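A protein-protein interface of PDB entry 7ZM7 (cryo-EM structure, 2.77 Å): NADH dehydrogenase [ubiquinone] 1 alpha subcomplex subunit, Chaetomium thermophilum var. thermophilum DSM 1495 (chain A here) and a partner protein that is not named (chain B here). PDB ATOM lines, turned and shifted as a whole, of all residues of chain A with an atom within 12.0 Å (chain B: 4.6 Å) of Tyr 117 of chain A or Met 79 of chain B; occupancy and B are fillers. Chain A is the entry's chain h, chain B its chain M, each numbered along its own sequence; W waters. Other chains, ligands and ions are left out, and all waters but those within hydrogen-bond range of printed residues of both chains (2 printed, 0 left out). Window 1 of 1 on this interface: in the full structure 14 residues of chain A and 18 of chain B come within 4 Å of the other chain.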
ATOM      1  N   ARG A 107     -18.622  14.061   2.803  1.00  0.00           N
ATOM      2  CA  ARG A 107     -17.990  12.809   3.162  1.00  0.00           C
ATOM      3  C   ARG A 107     -18.657  12.142   4.359  1.00  0.00           C
ATOM      4  O   ARG A 107     -18.072  11.263   4.988  1.00  0.00           O
ATOM      5  CB  ARG A 107     -16.478  13.061   3.297  1.00  0.00           C
ATOM      6  CG  ARG A 107     -15.644  11.878   3.609  1.00  0.00           C
ATOM      7  CD  ARG A 107     -14.189  12.206   3.604  1.00  0.00           C
ATOM      8  NE  ARG A 107     -13.786  12.487   2.241  1.00  0.00           N
ATOM      9  CZ  ARG A 107     -12.607  12.970   1.872  1.00  0.00           C
ATOM     10  NH1 ARG A 107     -12.354  13.148   0.584  1.00  0.00           N
ATOM     11  NH2 ARG A 107     -11.687  13.268   2.770  1.00  0.00           N
ATOM     12  N   ARG A 111     -16.766   6.201   6.112  1.00  0.00           N
ATOM     13  CA  ARG A 111     -15.814   6.105   7.210  1.00  0.00           C
ATOM     14  C   ARG A 111     -14.902   7.324   7.305  1.00  0.00           C
ATOM     15  O   ARG A 111     -14.196   7.479   8.303  1.00  0.00           O
ATOM     16  CB  ARG A 111     -15.012   4.813   7.043  1.00  0.00           C
ATOM     17  CG  ARG A 111     -14.068   4.462   8.156  1.00  0.00           C
ATOM     18  CD  ARG A 111     -13.694   2.996   8.107  1.00  0.00           C
ATOM     19  NE  ARG A 111     -14.844   2.124   8.277  1.00  0.00           N
ATOM     20  CZ  ARG A 111     -14.884   1.123   9.143  1.00  0.00           C
ATOM     21  NH1 ARG A 111     -15.970   0.377   9.257  1.00  0.00           N
ATOM     22  NH2 ARG A 111     -13.815   0.845   9.866  1.00  0.00           N
ATOM     23  N   GLY A 112     -14.908   8.194   6.307  1.00  0.00           N
ATOM     24  CA  GLY A 112     -14.193   9.445   6.370  1.00  0.00           C
ATOM     25  C   GLY A 112     -14.969  10.629   6.898  1.00  0.00           C
ATOM     26  O   GLY A 112     -14.510  11.759   6.738  1.00  0.00           O
ATOM     27  N   ALA A 113     -16.119  10.410   7.530  1.00  0.00           N
ATOM     28  CA  ALA A 113     -16.961  11.501   8.002  1.00  0.00           C
ATOM     29  C   ALA A 113     -16.276  12.308   9.095  1.00  0.00           C
ATOM     30  O   ALA A 113     -15.515  11.783   9.907  1.00  0.00           O
ATOM     31  CB  ALA A 113     -18.281  10.961   8.524  1.00  0.00           C
ATOM     32  N   TYR A 114     -16.577  13.605   9.112  1.00  0.00           N
ATOM     33  CA  TYR A 114     -15.934  14.535  10.025  1.00  0.00           C
ATOM     34  C   TYR A 114     -16.325  14.237  11.460  1.00  0.00           C
ATOM     35  O   TYR A 114     -17.496  14.021  11.765  1.00  0.00           O
ATOM     36  CB  TYR A 114     -16.305  15.969   9.654  1.00  0.00           C
ATOM     37  CG  TYR A 114     -16.251  16.950  10.796  1.00  0.00           C
ATOM     38  CD1 TYR A 114     -15.047  17.381  11.311  1.00  0.00           C
ATOM     39  CD2 TYR A 114     -17.408  17.433  11.358  1.00  0.00           C
ATOM     40  CE1 TYR A 114     -15.006  18.261  12.348  1.00  0.00           C
ATOM     41  CE2 TYR A 114     -17.378  18.305  12.386  1.00  0.00           C
ATOM     42  CZ  TYR A 114     -16.183  18.719  12.886  1.00  0.00           C
ATOM     43  OH  TYR A 114     -16.188  19.600  13.926  1.00  0.00           O
ATOM     44  N   LYS A 115     -15.341  14.255  12.345  1.00  0.00           N
ATOM     45  CA  LYS A 115     -15.549  14.001  13.758  1.00  0.00           C
ATOM     46  C   LYS A 115     -15.097  15.201  14.576  1.00  0.00           C
ATOM     47  O   LYS A 115     -13.915  15.566  14.534  1.00  0.00           O
ATOM     48  CB  LYS A 115     -14.803  12.734  14.171  1.00  0.00           C
ATOM     49  CG  LYS A 115     -15.387  11.506  13.534  1.00  0.00           C
ATOM     50  CD  LYS A 115     -14.715  10.258  13.959  1.00  0.00           C
ATOM     51  CE  LYS A 115     -15.318   9.102  13.215  1.00  0.00           C
ATOM     52  NZ  LYS A 115     -16.723   8.900  13.643  1.00  0.00           N
ATOM     53  N   PRO A 116     -15.989  15.856  15.298  1.00  0.00           N
ATOM     54  CA  PRO A 116     -15.593  17.019  16.088  1.00  0.00           C
ATOM     55  C   PRO A 116     -14.827  16.610  17.329  1.00  0.00           C
ATOM     56  O   PRO A 116     -14.903  15.478  17.803  1.00  0.00           O
ATOM     57  CB  PRO A 116     -16.933  17.654  16.449  1.00  0.00           C
ATOM     58  CG  PRO A 116     -17.830  16.512  16.542  1.00  0.00           C
ATOM     59  CD  PRO A 116     -17.420  15.578  15.442  1.00  0.00           C
ATOM     60  N   TYR A 117     -14.072  17.560  17.853  1.00  0.00           N
ATOM     61  CA  TYR A 117     -13.380  17.349  19.107  1.00  0.00           C
ATOM     62  C   TYR A 117     -13.122  18.696  19.754  1.00  0.00           C
ATOM     63  O   TYR A 117     -13.169  19.740  19.106  1.00  0.00           O
ATOM     64  CB  TYR A 117     -12.066  16.584  18.915  1.00  0.00           C
ATOM     65  CG  TYR A 117     -11.178  17.185  17.879  1.00  0.00           C
ATOM     66  CD1 TYR A 117     -10.327  18.226  18.186  1.00  0.00           C
ATOM     67  CD2 TYR A 117     -11.206  16.731  16.585  1.00  0.00           C
ATOM     68  CE1 TYR A 117      -9.526  18.780  17.248  1.00  0.00           C
ATOM     69  CE2 TYR A 117     -10.414  17.285  15.633  1.00  0.00           C
ATOM     70  CZ  TYR A 117      -9.571  18.310  15.970  1.00  0.00           C
ATOM     71  OH  TYR A 117      -8.775  18.863  15.012  1.00  0.00           O
ATOM     72  N   ASN A 118     -12.837  18.645  21.046  1.00  0.00           N
ATOM     73  CA  ASN A 118     -12.362  19.810  21.764  1.00  0.00           C
ATOM     74  C   ASN A 118     -11.002  20.228  21.230  1.00  0.00           C
ATOM     75  O   ASN A 118     -10.134  19.400  20.975  1.00  0.00           O
ATOM     76  CB  ASN A 118     -12.278  19.503  23.252  1.00  0.00           C
ATOM     77  CG  ASN A 118     -12.256  20.748  24.105  1.00  0.00           C
ATOM     78  OD1 ASN A 118     -12.293  21.860  23.609  1.00  0.00           O
ATOM     79  ND2 ASN A 118     -12.206  20.561  25.402  1.00  0.00           N
ATOM     80  N   THR A 119     -10.825  21.528  21.059  1.00  0.00           N
ATOM     81  CA  THR A 119      -9.594  22.106  20.558  1.00  0.00           C
ATOM     82  C   THR A 119      -8.767  22.742  21.671  1.00  0.00           C
ATOM     83  O   THR A 119      -7.594  23.054  21.458  1.00  0.00           O
ATOM     84  CB  THR A 119      -9.947  23.123  19.450  1.00  0.00           C
ATOM     85  OG1 THR A 119     -10.543  22.435  18.347  1.00  0.00           O
ATOM     86  CG2 THR A 119      -8.763  23.833  18.924  1.00  0.00           C
ATOM     87  N   THR A 120      -9.329  22.879  22.870  1.00  0.00           N
ATOM     88  CA  THR A 120      -8.677  23.529  23.995  1.00  0.00           C
ATOM     89  C   THR A 120      -8.272  22.516  25.061  1.00  0.00           C
ATOM     90  O   THR A 120      -8.776  21.397  25.100  1.00  0.00           O
ATOM     91  CB  THR A 120      -9.585  24.610  24.605  1.00  0.00           C
ATOM     92  OG1 THR A 120     -10.823  24.045  25.035  1.00  0.00           O
ATOM     93  CG2 THR A 120      -9.884  25.667  23.606  1.00  0.00           C
ATOM     94  N   GLN A 121      -7.328  22.924  25.911  1.00  0.00           N
ATOM     95  CA  GLN A 121      -6.802  22.080  26.976  1.00  0.00           C
ATOM     96  C   GLN A 121      -7.736  22.061  28.188  1.00  0.00           C
ATOM     97  O   GLN A 121      -8.559  22.956  28.365  1.00  0.00           O
ATOM     98  CB  GLN A 121      -5.426  22.576  27.398  1.00  0.00           C
ATOM     99  CG  GLN A 121      -4.382  22.505  26.328  1.00  0.00           C
ATOM    100  CD  GLN A 121      -3.596  21.216  26.346  1.00  0.00           C
ATOM    101  OE1 GLN A 121      -4.150  20.133  26.218  1.00  0.00           O
ATOM    102  NE2 GLN A 121      -2.296  21.327  26.491  1.00  0.00           N
ATOM    103  N   PRO A 122      -7.640  21.033  29.028  1.00  0.00           N
ATOM    104  CA  PRO A 122      -8.459  20.997  30.247  1.00  0.00           C
ATOM    105  C   PRO A 122      -8.179  22.183  31.150  1.00  0.00           C
ATOM    106  O   PRO A 122      -7.034  22.610  31.308  1.00  0.00           O
ATOM    107  CB  PRO A 122      -8.056  19.688  30.917  1.00  0.00           C
ATOM    108  CG  PRO A 122      -7.291  18.937  29.921  1.00  0.00           C
ATOM    109  CD  PRO A 122      -6.852  19.809  28.836  1.00  0.00           C
ATOM    110  N   THR B  51      -5.818   5.891  15.796  1.00  0.00           N
ATOM    111  CA  THR B  51      -4.939   7.036  15.986  1.00  0.00           C
ATOM    112  C   THR B  51      -3.472   6.627  16.009  1.00  0.00           C
ATOM    113  O   THR B  51      -3.144   5.442  15.989  1.00  0.00           O
ATOM    114  CB  THR B  51      -5.258   7.776  17.287  1.00  0.00           C
ATOM    115  OG1 THR B  51      -4.322   8.845  17.466  1.00  0.00           O
ATOM    116  CG2 THR B  51      -5.161   6.832  18.472  1.00  0.00           C
ATOM    117  N   ALA B  57      -3.041  12.305  11.969  1.00  0.00           N
ATOM    118  CA  ALA B  57      -3.513  12.239  13.341  1.00  0.00           C
ATOM    119  C   ALA B  57      -2.468  12.687  14.357  1.00  0.00           C
ATOM    120  O   ALA B  57      -2.798  12.835  15.534  1.00  0.00           O
ATOM    121  CB  ALA B  57      -3.964  10.816  13.664  1.00  0.00           C
ATOM    122  N   ARG B  75      -3.425  17.461  18.493  1.00  0.00           N
ATOM    123  CA  ARG B  75      -4.282  16.540  17.757  1.00  0.00           C
ATOM    124  C   ARG B  75      -4.094  15.107  18.221  1.00  0.00           C
ATOM    125  O   ARG B  75      -4.996  14.282  18.072  1.00  0.00           O
ATOM    126  CB  ARG B  75      -4.005  16.589  16.262  1.00  0.00           C
ATOM    127  CG  ARG B  75      -4.245  17.868  15.588  1.00  0.00           C
ATOM    128  CD  ARG B  75      -4.051  17.658  14.124  1.00  0.00           C
ATOM    129  NE  ARG B  75      -5.164  16.927  13.552  1.00  0.00           N
ATOM    130  CZ  ARG B  75      -6.214  17.518  13.000  1.00  0.00           C
ATOM    131  NH1 ARG B  75      -7.194  16.798  12.496  1.00  0.00           N
ATOM    132  NH2 ARG B  75      -6.273  18.835  12.942  1.00  0.00           N
ATOM    133  N   SER B  76      -2.913  14.786  18.735  1.00  0.00           N
ATOM    134  CA  SER B  76      -2.673  13.464  19.278  1.00  0.00           C
ATOM    135  C   SER B  76      -3.608  13.171  20.440  1.00  0.00           C
ATOM    136  O   SER B  76      -4.085  12.044  20.595  1.00  0.00           O
ATOM    137  CB  SER B  76      -1.218  13.361  19.712  1.00  0.00           C
ATOM    138  OG  SER B  76      -0.365  13.487  18.595  1.00  0.00           O
ATOM    139  N   GLU B  77      -3.883  14.171  21.267  1.00  0.00           N
ATOM    140  CA  GLU B  77      -4.746  13.952  22.416  1.00  0.00           C
ATOM    141  C   GLU B  77      -6.202  14.232  22.089  1.00  0.00           C
ATOM    142  O   GLU B  77      -7.094  13.692  22.747  1.00  0.00           O
ATOM    143  CB  GLU B  77      -4.281  14.819  23.579  1.00  0.00           C
ATOM    144  CG  GLU B  77      -2.926  14.424  24.090  1.00  0.00           C
ATOM    145  CD  GLU B  77      -2.926  13.043  24.729  1.00  0.00           C
ATOM    146  OE1 GLU B  77      -3.958  12.647  25.313  1.00  0.00           O
ATOM    147  OE2 GLU B  77      -1.895  12.346  24.630  1.00  0.00           O
ATOM    148  N   ALA B  78      -6.456  15.074  21.089  1.00  0.00           N
ATOM    149  CA  ALA B  78      -7.820  15.383  20.689  1.00  0.00           C
ATOM    150  C   ALA B  78      -8.441  14.247  19.910  1.00  0.00           C
ATOM    151  O   ALA B  78      -9.656  14.043  19.973  1.00  0.00           O
ATOM    152  CB  ALA B  78      -7.842  16.647  19.849  1.00  0.00           C
ATOM    153  N   MET B  79      -7.624  13.506  19.170  1.00  0.00           N
ATOM    154  CA  MET B  79      -8.072  12.429  18.305  1.00  0.00           C
ATOM    155  C   MET B  79      -7.639  11.077  18.841  1.00  0.00           C
ATOM    156  O   MET B  79      -7.351  10.163  18.068  1.00  0.00           O
ATOM    157  CB  MET B  79      -7.559  12.654  16.883  1.00  0.00           C
ATOM    158  CG  MET B  79      -7.893  14.029  16.344  1.00  0.00           C
ATOM    159  SD  MET B  79      -7.289  14.305  14.677  1.00  0.00           S
ATOM    160  CE  MET B  79      -8.796  14.193  13.746  1.00  0.00           C
ATOM    161  N   ALA B  80      -7.543  10.954  20.155  1.00  0.00           N
ATOM    162  CA  ALA B  80      -7.476   9.668  20.825  1.00  0.00           C
ATOM    163  C   ALA B  80      -8.862   9.315  21.343  1.00  0.00           C
ATOM    164  O   ALA B  80      -9.742  10.167  21.440  1.00  0.00           O
ATOM    165  CB  ALA B  80      -6.466   9.699  21.968  1.00  0.00           C
ATOM    166  N   GLY B  81      -9.067   8.047  21.647  1.00  0.00           N
ATOM    167  CA  GLY B  81     -10.325   7.631  22.220  1.00  0.00           C
ATOM    168  C   GLY B  81     -11.202   6.823  21.286  1.00  0.00           C
ATOM    169  O   GLY B  81     -10.873   6.584  20.123  1.00  0.00           O
ATOM    170  N   ARG B  83     -14.169   7.385  19.773  1.00  0.00           N
ATOM    171  CA  ARG B  83     -14.854   7.955  18.616  1.00  0.00           C
ATOM    172  C   ARG B  83     -13.984   7.967  17.367  1.00  0.00           C
ATOM    173  O   ARG B  83     -14.516   8.066  16.261  1.00  0.00           O
ATOM    174  CB  ARG B  83     -15.342   9.379  18.899  1.00  0.00           C
ATOM    175  CG  ARG B  83     -16.443   9.496  19.921  1.00  0.00           C
ATOM    176  CD  ARG B  83     -17.040  10.914  20.001  1.00  0.00           C
ATOM    177  NE  ARG B  83     -16.067  11.951  20.357  1.00  0.00           N
ATOM    178  CZ  ARG B  83     -15.624  12.885  19.520  1.00  0.00           C
ATOM    179  NH1 ARG B  83     -14.746  13.773  19.930  1.00  0.00           N
ATOM    180  NH2 ARG B  83     -16.041  12.920  18.268  1.00  0.00           N
ATOM    181  N   PHE B  84     -12.667   7.881  17.510  1.00  0.00           N
ATOM    182  CA  PHE B  84     -11.767   7.984  16.376  1.00  0.00           C
ATOM    183  C   PHE B  84     -11.236   6.629  15.937  1.00  0.00           C
ATOM    184  O   PHE B  84     -10.230   6.561  15.229  1.00  0.00           O
ATOM    185  CB  PHE B  84     -10.640   8.960  16.705  1.00  0.00           C
ATOM    186  CG  PHE B  84     -11.109  10.372  16.823  1.00  0.00           C
ATOM    187  CD1 PHE B  84     -11.212  11.178  15.710  1.00  0.00           C
ATOM    188  CD2 PHE B  84     -11.482  10.890  18.045  1.00  0.00           C
ATOM    189  CE1 PHE B  84     -11.672  12.460  15.812  1.00  0.00           C
ATOM    190  CE2 PHE B  84     -11.939  12.185  18.154  1.00  0.00           C
ATOM    191  CZ  PHE B  84     -12.033  12.970  17.035  1.00  0.00           C
ATOM    192  N   PHE B  89      -8.362   9.176   9.014  1.00  0.00           N
ATOM    193  CA  PHE B  89      -7.748  10.398   9.508  1.00  0.00           C
ATOM    194  C   PHE B  89      -7.253  11.297   8.398  1.00  0.00           C
ATOM    195  O   PHE B  89      -6.916  12.451   8.660  1.00  0.00           O
ATOM    196  CB  PHE B  89      -6.582  10.071  10.435  1.00  0.00           C
ATOM    197  CG  PHE B  89      -7.008   9.589  11.769  1.00  0.00           C
ATOM    198  CD1 PHE B  89      -7.711  10.412  12.625  1.00  0.00           C
ATOM    199  CD2 PHE B  89      -6.721   8.307  12.171  1.00  0.00           C
ATOM    200  CE1 PHE B  89      -8.113   9.953  13.857  1.00  0.00           C
ATOM    201  CE2 PHE B  89      -7.116   7.855  13.400  1.00  0.00           C
ATOM    202  CZ  PHE B  89      -7.807   8.672  14.244  1.00  0.00           C
ATOM    203  N   GLN B  92     -10.046  13.744   7.688  1.00  0.00           N
ATOM    204  CA  GLN B  92     -10.368  14.685   8.775  1.00  0.00           C
ATOM    205  C   GLN B  92      -9.980  16.104   8.363  1.00  0.00           C
ATOM    206  O   GLN B  92      -8.948  16.258   7.703  1.00  0.00           O
ATOM    207  CB  GLN B  92      -9.789  14.130  10.075  1.00  0.00           C
ATOM    208  CG  GLN B  92     -10.507  12.879  10.558  1.00  0.00           C
ATOM    209  CD  GLN B  92     -12.006  13.042  10.580  1.00  0.00           C
ATOM    210  OE1 GLN B  92     -12.540  14.002  11.132  1.00  0.00           O
ATOM    211  NE2 GLN B  92     -12.701  12.093   9.976  1.00  0.00           N
HETATM  212  O   HOH W   1     -13.201  15.515  21.963  1.00  0.00           O
HETATM  213  O   HOH W   2      -6.228  20.369  15.513  1.00  0.00           O
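Printed residues of chain A that touch a printed residue of chain B: Gly 112, Ala 113, Tyr 114, Lys 115, Pro 116, Tyr 117 and Asn 118. Hydrophobic or aromatic side chains of chain A within 4 Å of the printed part of chain B: Tyr 117. Of the 13 printed residues of chain B, 6 touch a printed residue of chain A. Hydrophobic or aromatic side chains of chain B within 4 Å of the printed part of chain A: Ala 78, Met 79 and Phe 84. Among the printed residues, no Asp or Glu carboxylate lies within 4 Å of a Lys or Arg side-chain nitrogen of the other chain.
The side-chain sulfur (SD) of Met 79 of chain B lies close to the guanidinium group (NH1) of Arg 75 of chain B (3.3 Å). OG1 of Thr 51 of chain B lies close to O of Met 79 of chain B. OD1 of Asn 118 of chain A is in hydrogen-bond range of OG1 of Thr 120 of chain A, 3.0 Å away. N of Ala 113 of chain A sits close to O of Arg 107 of chain A, 3.3 Å away.
Gly 112 of chain A touches Gln 92 of chain B. Gln 92 of chain B touches Tyr 114 of chain A (OE1 to CA, 3.6 Å). Arg 83 of chain B touches Lys 115 of chain A. Lys 115 of chain A touches Phe 84 of chain B. Pro 116 of chain A touches Phe 84 of chain B (O to CZ, 3.9 Å). Tyr 117 of chain A touches Ala 78 of chain B (CD1 to CB, 3.4 Å). Met 79 of chain B touches Tyr 117 of chain A (CE to CE2, 3.97 Å). CA of Tyr 117 of chain A touches NH1 of Arg 83 of chain B, at 3.9 Å. CZ of Phe 84 of chain B touches CD2 of Tyr 117 of chain A, at 3.9 Å. O of Asn 118 of chain A touches CB of Ala 78 of chain B, at 3.8 Å.
Water W2 lies within hydrogen-bond range of NH2 of Arg 75 of chain B and OH of Tyr 117 of chain A. Water W1 bridges the guanidinium group (NH1) of Arg 83 of chain B (3.1 Å) and the backbone NH (N) of Asn 118 of chain A (3.3 Å).
Of the printed residues of chain B, Tyr 117 of chain A touches Arg 75 (3.2 Å), Ala 78 (3.4 Å), Met 79 (3.97 Å), Arg 83 (3.9 Å) and Phe 84 (3.9 Å). Met 79 of chain B touches one residue of chain A. No residue of chain A comes within 4 Å of Thr 51 of chain B. No residue of chain A comes within 4 Å of Ala 57 of chain B. Of chain A, only Tyr 117 comes within 4 Å of Arg 75 of chain B. No residue of chain A comes within 4 Å of Ser 76 of chain B. Ala 80 of chain B touches none of the printed residues of chain A. Of chain A, only Lys 115 (3.5 Å), Pro 116 (3.9 Å) and Tyr 117 (3.9 Å) come within 4 Å of Phe 84 of chain B. Gln 92 of chain B touches just these residues of chain A: Gly 112 (3.7 Å), Ala 113 (2.8 Å), Tyr 114 (3.6 Å) and Lys 115 (3.1 Å). Of the printed residues of chain B, Tyr 114 of chain A touches Gln 92 (3.6 Å). Of the printed residues of chain A, Arg 83 of chain B touches Lys 115, Pro 116 and Tyr 117. Printed residues of chain B within 4 Å of Gly 112 of chain A: Gln 92. The nearest printed residue of chain B that does not touch Tyr 117 of chain A is Gln 92 of chain B (6.0 Å).
N of Lys 115 of chain A is in hydrogen-bond range of OE1 of Gln 92 of chain B. NE2 of Gln 92 of chain B sits at hydrogen-bond distance from O of Ala 113 of chain A (2.8 Å). NH2 of Arg 75 of chain B is in hydrogen-bond range of OH of Tyr 117 of chain A (3.2 Å). The guanidinium group (NH1) of Arg 83 of chain B is in hydrogen-bond range of the backbone carbonyl oxygen (O) of Pro 116 of chain A.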
